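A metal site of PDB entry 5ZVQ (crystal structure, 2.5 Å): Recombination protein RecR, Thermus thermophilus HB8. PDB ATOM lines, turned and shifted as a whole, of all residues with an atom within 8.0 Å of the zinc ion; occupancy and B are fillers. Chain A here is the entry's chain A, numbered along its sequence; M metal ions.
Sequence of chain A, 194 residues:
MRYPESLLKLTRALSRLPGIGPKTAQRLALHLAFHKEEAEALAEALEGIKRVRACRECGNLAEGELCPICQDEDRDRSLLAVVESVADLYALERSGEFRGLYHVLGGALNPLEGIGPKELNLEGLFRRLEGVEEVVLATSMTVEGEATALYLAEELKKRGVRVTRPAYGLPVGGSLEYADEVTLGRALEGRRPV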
ATOM      1  N   ALA A  54      23.338 -11.074  -7.764  1.00  0.00           N
ATOM      2  CA  ALA A  54      22.024 -11.715  -7.654  1.00  0.00           C
ATOM      3  C   ALA A  54      20.938 -10.694  -7.962  1.00  0.00           C
ATOM      4  O   ALA A  54      21.031  -9.546  -7.549  1.00  0.00           O
ATOM      5  CB  ALA A  54      21.830 -12.294  -6.272  1.00  0.00           C
ATOM      6  N   CYS A  55      19.920 -11.122  -8.719  1.00  0.00           N
ATOM      7  CA  CYS A  55      18.785 -10.278  -9.025  1.00  0.00           C
ATOM      8  C   CYS A  55      17.973 -10.016  -7.760  1.00  0.00           C
ATOM      9  O   CYS A  55      17.799 -10.904  -6.926  1.00  0.00           O
ATOM     10  CB  CYS A  55      17.886 -10.933 -10.077  1.00  0.00           C
ATOM     11  SG  CYS A  55      16.327 -10.095 -10.449  1.00  0.00           S
ATOM     12  N   ARG A  56      17.481  -8.782  -7.649  1.00  0.00           N
ATOM     13  CA  ARG A  56      16.721  -8.326  -6.483  1.00  0.00           C
ATOM     14  C   ARG A  56      15.499  -9.201  -6.188  1.00  0.00           C
ATOM     15  O   ARG A  56      15.126  -9.369  -5.033  1.00  0.00           O
ATOM     16  CB  ARG A  56      16.295  -6.862  -6.700  1.00  0.00           C
ATOM     17  CG  ARG A  56      15.700  -6.164  -5.490  1.00  0.00           C
ATOM     18  CD  ARG A  56      15.809  -4.642  -5.640  1.00  0.00           C
ATOM     19  NE  ARG A  56      15.272  -4.176  -6.924  1.00  0.00           N
ATOM     20  CZ  ARG A  56      15.550  -2.992  -7.495  1.00  0.00           C
ATOM     21  NH1 ARG A  56      16.368  -2.115  -6.916  1.00  0.00           N
ATOM     22  NH2 ARG A  56      15.005  -2.697  -8.678  1.00  0.00           N
ATOM     23  N   GLU A  57      14.909  -9.766  -7.244  1.00  0.00           N
ATOM     24  CA  GLU A  57      13.690 -10.565  -7.150  1.00  0.00           C
ATOM     25  C   GLU A  57      13.939 -12.087  -7.309  1.00  0.00           C
ATOM     26  O   GLU A  57      13.500 -12.859  -6.456  1.00  0.00           O
ATOM     27  CB  GLU A  57      12.669 -10.038  -8.176  1.00  0.00           C
ATOM     28  CG  GLU A  57      11.316  -9.631  -7.592  1.00  0.00           C
ATOM     29  CD  GLU A  57      11.387  -8.383  -6.730  1.00  0.00           C
ATOM     30  OE1 GLU A  57      11.862  -8.465  -5.574  1.00  0.00           O
ATOM     31  OE2 GLU A  57      10.936  -7.304  -7.191  1.00  0.00           O
ATOM     32  N   CYS A  58      14.656 -12.494  -8.361  1.00  0.00           N
ATOM     33  CA  CYS A  58      14.916 -13.935  -8.638  1.00  0.00           C
ATOM     34  C   CYS A  58      15.963 -14.595  -7.761  1.00  0.00           C
ATOM     35  O   CYS A  58      15.722 -15.659  -7.210  1.00  0.00           O
ATOM     36  CB  CYS A  58      15.434 -14.157 -10.070  1.00  0.00           C
ATOM     37  SG  CYS A  58      14.258 -14.205 -11.418  1.00  0.00           S
ATOM     38  N   GLY A  59      17.132 -13.964  -7.669  1.00  0.00           N
ATOM     39  CA  GLY A  59      18.369 -14.649  -7.309  1.00  0.00           C
ATOM     40  C   GLY A  59      19.172 -15.126  -8.522  1.00  0.00           C
ATOM     41  O   GLY A  59      20.184 -15.817  -8.373  1.00  0.00           O
ATOM     42  N   ASN A  60      18.736 -14.716  -9.711  1.00  0.00           N
ATOM     43  CA  ASN A  60      19.360 -15.068 -10.981  1.00  0.00           C
ATOM     44  C   ASN A  60      20.430 -14.015 -11.253  1.00  0.00           C
ATOM     45  O   ASN A  60      20.313 -12.882 -10.777  1.00  0.00           O
ATOM     46  CB  ASN A  60      18.283 -15.094 -12.087  1.00  0.00           C
ATOM     47  CG  ASN A  60      18.823 -15.465 -13.457  1.00  0.00           C
ATOM     48  OD1 ASN A  60      19.940 -15.958 -13.603  1.00  0.00           O
ATOM     49  ND2 ASN A  60      18.021 -15.213 -14.488  1.00  0.00           N
ATOM     50  N   LEU A  61      21.469 -14.378 -12.002  1.00  0.00           N
ATOM     51  CA  LEU A  61      22.549 -13.436 -12.295  1.00  0.00           C
ATOM     52  C   LEU A  61      22.054 -12.269 -13.154  1.00  0.00           C
ATOM     53  O   LEU A  61      21.334 -12.484 -14.136  1.00  0.00           O
ATOM     54  CB  LEU A  61      23.721 -14.141 -12.994  1.00  0.00           C
ATOM     55  CG  LEU A  61      24.514 -15.151 -12.155  1.00  0.00           C
ATOM     56  CD1 LEU A  61      25.756 -15.565 -12.937  1.00  0.00           C
ATOM     57  CD2 LEU A  61      24.917 -14.606 -10.795  1.00  0.00           C
ATOM     58  N   ALA A  62      22.469 -11.060 -12.771  1.00  0.00           N
ATOM     59  CA  ALA A  62      21.922  -9.824 -13.329  1.00  0.00           C
ATOM     60  C   ALA A  62      22.972  -8.719 -13.467  1.00  0.00           C
ATOM     61  O   ALA A  62      23.852  -8.572 -12.611  1.00  0.00           O
ATOM     62  CB  ALA A  62      20.783  -9.342 -12.449  1.00  0.00           C
ATOM     63  N   GLU A  65      20.561  -4.414 -11.174  1.00  0.00           N
ATOM     64  CA  GLU A  65      19.458  -4.678 -10.253  1.00  0.00           C
ATOM     65  C   GLU A  65      18.632  -5.919 -10.624  1.00  0.00           C
ATOM     66  O   GLU A  65      18.565  -6.869  -9.840  1.00  0.00           O
ATOM     67  CB  GLU A  65      18.534  -3.456 -10.166  1.00  0.00           C
ATOM     68  N   LEU A  66      18.006  -5.879 -11.799  1.00  0.00           N
ATOM     69  CA  LEU A  66      17.080  -6.933 -12.251  1.00  0.00           C
ATOM     70  C   LEU A  66      17.697  -7.810 -13.344  1.00  0.00           C
ATOM     71  O   LEU A  66      18.418  -7.303 -14.204  1.00  0.00           O
ATOM     72  CB  LEU A  66      15.776  -6.311 -12.772  1.00  0.00           C
ATOM     73  CG  LEU A  66      14.973  -5.441 -11.801  1.00  0.00           C
ATOM     74  CD1 LEU A  66      13.820  -4.767 -12.535  1.00  0.00           C
ATOM     75  CD2 LEU A  66      14.458  -6.247 -10.623  1.00  0.00           C
ATOM     76  N   CYS A  67      17.409  -9.116 -13.304  1.00  0.00           N
ATOM     77  CA  CYS A  67      17.903 -10.059 -14.309  1.00  0.00           C
ATOM     78  C   CYS A  67      17.175  -9.860 -15.641  1.00  0.00           C
ATOM     79  O   CYS A  67      16.079  -9.271 -15.651  1.00  0.00           O
ATOM     80  CB  CYS A  67      17.744 -11.515 -13.837  1.00  0.00           C
ATOM     81  SG  CYS A  67      16.054 -12.153 -13.834  1.00  0.00           S
ATOM     82  N   PRO A  68      17.752 -10.344 -16.759  1.00  0.00           N
ATOM     83  CA  PRO A  68      17.090 -10.204 -18.055  1.00  0.00           C
ATOM     84  C   PRO A  68      15.681 -10.815 -18.137  1.00  0.00           C
ATOM     85  O   PRO A  68      14.852 -10.316 -18.906  1.00  0.00           O
ATOM     86  CB  PRO A  68      18.017 -10.942 -19.019  1.00  0.00           C
ATOM     87  CG  PRO A  68      19.349 -10.904 -18.357  1.00  0.00           C
ATOM     88  CD  PRO A  68      19.055 -11.017 -16.890  1.00  0.00           C
ATOM     89  N   ILE A  69      15.432 -11.876 -17.361  1.00  0.00           N
ATOM     90  CA  ILE A  69      14.119 -12.521 -17.343  1.00  0.00           C
ATOM     91  C   ILE A  69      13.080 -11.596 -16.683  1.00  0.00           C
ATOM     92  O   ILE A  69      12.015 -11.356 -17.260  1.00  0.00           O
ATOM     93  CB  ILE A  69      14.167 -13.899 -16.647  1.00  0.00           C
ATOM     94  CG1 ILE A  69      15.101 -14.850 -17.407  1.00  0.00           C
ATOM     95  CG2 ILE A  69      12.776 -14.514 -16.547  1.00  0.00           C
ATOM     96  N   CYS A  70      13.391 -11.077 -15.495  1.00  0.00           N
ATOM     97  CA  CYS A  70      12.439 -10.235 -14.744  1.00  0.00           C
ATOM     98  C   CYS A  70      12.075  -8.924 -15.442  1.00  0.00           C
ATOM     99  O   CYS A  70      10.919  -8.490 -15.386  1.00  0.00           O
ATOM    100  CB  CYS A  70      12.969  -9.938 -13.336  1.00  0.00           C
ATOM    101  SG  CYS A  70      12.953 -11.381 -12.260  1.00  0.00           S
ATOM    102  N   GLN A  71      13.047  -8.301 -16.104  1.00  0.00           N
ATOM    103  CA  GLN A  71      12.815  -7.074 -16.867  1.00  0.00           C
ATOM    104  C   GLN A  71      12.453  -7.294 -18.353  1.00  0.00           C
ATOM    105  O   GLN A  71      12.543  -6.374 -19.165  1.00  0.00           O
ATOM    106  CB  GLN A  71      14.011  -6.118 -16.717  1.00  0.00           C
ATOM    107  CG  GLN A  71      15.242  -6.451 -17.534  1.00  0.00           C
ATOM    108  CD  GLN A  71      16.478  -5.690 -17.076  1.00  0.00           C
ATOM    109  OE1 GLN A  71      17.604  -6.126 -17.324  1.00  0.00           O
ATOM    110  NE2 GLN A  71      16.277  -4.555 -16.411  1.00  0.00           N
ATOM    111  N   LEU A  89      18.191 -22.907 -14.107  1.00  0.00           N
ATOM    112  CA  LEU A  89      17.358 -21.884 -14.747  1.00  0.00           C
ATOM    113  C   LEU A  89      17.726 -21.803 -16.224  1.00  0.00           C
ATOM    114  O   LEU A  89      16.848 -21.878 -17.077  1.00  0.00           O
ATOM    115  CB  LEU A  89      17.572 -20.527 -14.058  1.00  0.00           C
ATOM    116  CG  LEU A  89      16.732 -19.306 -14.466  1.00  0.00           C
ATOM    117  CD1 LEU A  89      16.495 -18.402 -13.272  1.00  0.00           C
ATOM    118  CD2 LEU A  89      17.370 -18.519 -15.605  1.00  0.00           C
ATOM    119  N   LEU A 101       8.185 -16.864 -15.061  1.00  0.00           N
ATOM    120  CA  LEU A 101       9.262 -16.293 -14.241  1.00  0.00           C
ATOM    121  C   LEU A 101       9.924 -17.408 -13.433  1.00  0.00           C
ATOM    122  O   LEU A 101       9.429 -18.542 -13.399  1.00  0.00           O
ATOM    123  CB  LEU A 101       8.714 -15.204 -13.307  1.00  0.00           C
ATOM    124  CG  LEU A 101       8.198 -13.915 -13.959  1.00  0.00           C
ATOM    125  CD1 LEU A 101       7.411 -13.086 -12.955  1.00  0.00           C
ATOM    126  CD2 LEU A 101       9.330 -13.094 -14.563  1.00  0.00           C
ATOM    127  N   TYR A 102      11.035 -17.091 -12.785  1.00  0.00           N
ATOM    128  CA  TYR A 102      11.792 -18.047 -11.985  1.00  0.00           C
ATOM    129  C   TYR A 102      12.015 -17.510 -10.574  1.00  0.00           C
ATOM    130  O   TYR A 102      12.097 -16.300 -10.383  1.00  0.00           O
ATOM    131  CB  TYR A 102      13.160 -18.286 -12.600  1.00  0.00           C
ATOM    132  CG  TYR A 102      13.148 -18.931 -13.964  1.00  0.00           C
ATOM    133  CD1 TYR A 102      12.933 -20.301 -14.105  1.00  0.00           C
ATOM    134  CD2 TYR A 102      13.364 -18.172 -15.100  1.00  0.00           C
ATOM    135  CE1 TYR A 102      12.928 -20.904 -15.359  1.00  0.00           C
ATOM    136  CE2 TYR A 102      13.361 -18.754 -16.361  1.00  0.00           C
ATOM    137  CZ  TYR A 102      13.148 -20.127 -16.482  1.00  0.00           C
ATOM    138  OH  TYR A 102      13.149 -20.702 -17.732  1.00  0.00           O
ATOM    139  N   HIS A 103      12.136 -18.412  -9.609  1.00  0.00           N
ATOM    140  CA  HIS A 103      12.712 -18.085  -8.301  1.00  0.00           C
ATOM    141  C   HIS A 103      13.884 -19.005  -8.011  1.00  0.00           C
ATOM    142  O   HIS A 103      13.721 -20.229  -7.975  1.00  0.00           O
ATOM    143  CB  HIS A 103      11.684 -18.204  -7.164  1.00  0.00           C
ATOM    144  CG  HIS A 103      12.194 -17.647  -5.870  1.00  0.00           C
ATOM    145  ND1 HIS A 103      12.264 -16.291  -5.620  1.00  0.00           N
ATOM    146  CD2 HIS A 103      12.700 -18.259  -4.775  1.00  0.00           C
ATOM    147  CE1 HIS A 103      12.768 -16.097  -4.415  1.00  0.00           C
ATOM    148  NE2 HIS A 103      13.046 -17.282  -3.880  1.00  0.00           N
ATOM    149  N   VAL A 104      15.064 -18.423  -7.828  1.00  0.00           N
ATOM    150  CA  VAL A 104      16.292 -19.191  -7.635  1.00  0.00           C
ATOM    151  C   VAL A 104      16.589 -19.321  -6.140  1.00  0.00           C
ATOM    152  O   VAL A 104      16.876 -18.326  -5.462  1.00  0.00           O
ATOM    153  CB  VAL A 104      17.489 -18.570  -8.394  1.00  0.00           C
ATOM    154  CG1 VAL A 104      18.788 -19.292  -8.065  1.00  0.00           C
ATOM    155  CG2 VAL A 104      17.235 -18.612  -9.894  1.00  0.00           C
ATOM    156  N   ARG A 128       6.109 -12.957  -3.801  1.00  0.00           N
ATOM    157  CA  ARG A 128       5.919 -12.761  -5.250  1.00  0.00           C
ATOM    158  C   ARG A 128       4.763 -13.570  -5.866  1.00  0.00           C
ATOM    159  O   ARG A 128       4.783 -13.858  -7.063  1.00  0.00           O
ATOM    160  CB  ARG A 128       7.203 -13.127  -5.996  1.00  0.00           C
ATOM    161  CG  ARG A 128       8.488 -12.705  -5.299  1.00  0.00           C
ATOM    162  CD  ARG A 128       9.601 -12.569  -6.326  1.00  0.00           C
ATOM    163  NE  ARG A 128       9.798 -13.803  -7.070  1.00  0.00           N
ATOM    164  CZ  ARG A 128      10.250 -13.910  -8.323  1.00  0.00           C
ATOM    165  NH1 ARG A 128      10.369 -15.115  -8.863  1.00  0.00           N
ATOM    166  NH2 ARG A 128      10.585 -12.842  -9.053  1.00  0.00           N
HETATM  167 ZN    ZN M   1      15.210 -11.879 -11.657  1.00  0.00          ZN
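The side-chain sulfur (SG) of Cys 67 sits close to the side-chain amide nitrogen (ND2) of Asn 60, 3.7 Å away.
The side-chain sulfur (SG) of Cys 67 lies close to the backbone NH (N) of Ile 69 (3.6 Å).
The backbone NH (N) of Cys 55 is in hydrogen-bond range of the backbone carbonyl oxygen (O) of Asn 60 (2.7 Å).
N of Glu 57 lies close to SG of Cys 55 (3.5 Å).
The backbone carbonyl oxygen (O) of Tyr 102 sits close to the side-chain sulfur (SG) of Cys 58 (3.2 Å).
The backbone carbonyl oxygen (O) of Cys 58 lies within hydrogen-bond range of the backbone NH (N) of Val 104 (2.9 Å).
Of the 22 residues printed, 4 come within 4 Å of the zinc ion.
SG of Cys 67 is bound to the zinc ion, at 2.4 Å.
SG of Cys 70 binds the zinc ion.
SG of Cys 55 is bound to the zinc ion, 2.4 Å away.
SG of Cys 58 is bound to the zinc ion, at 2.5 Å.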
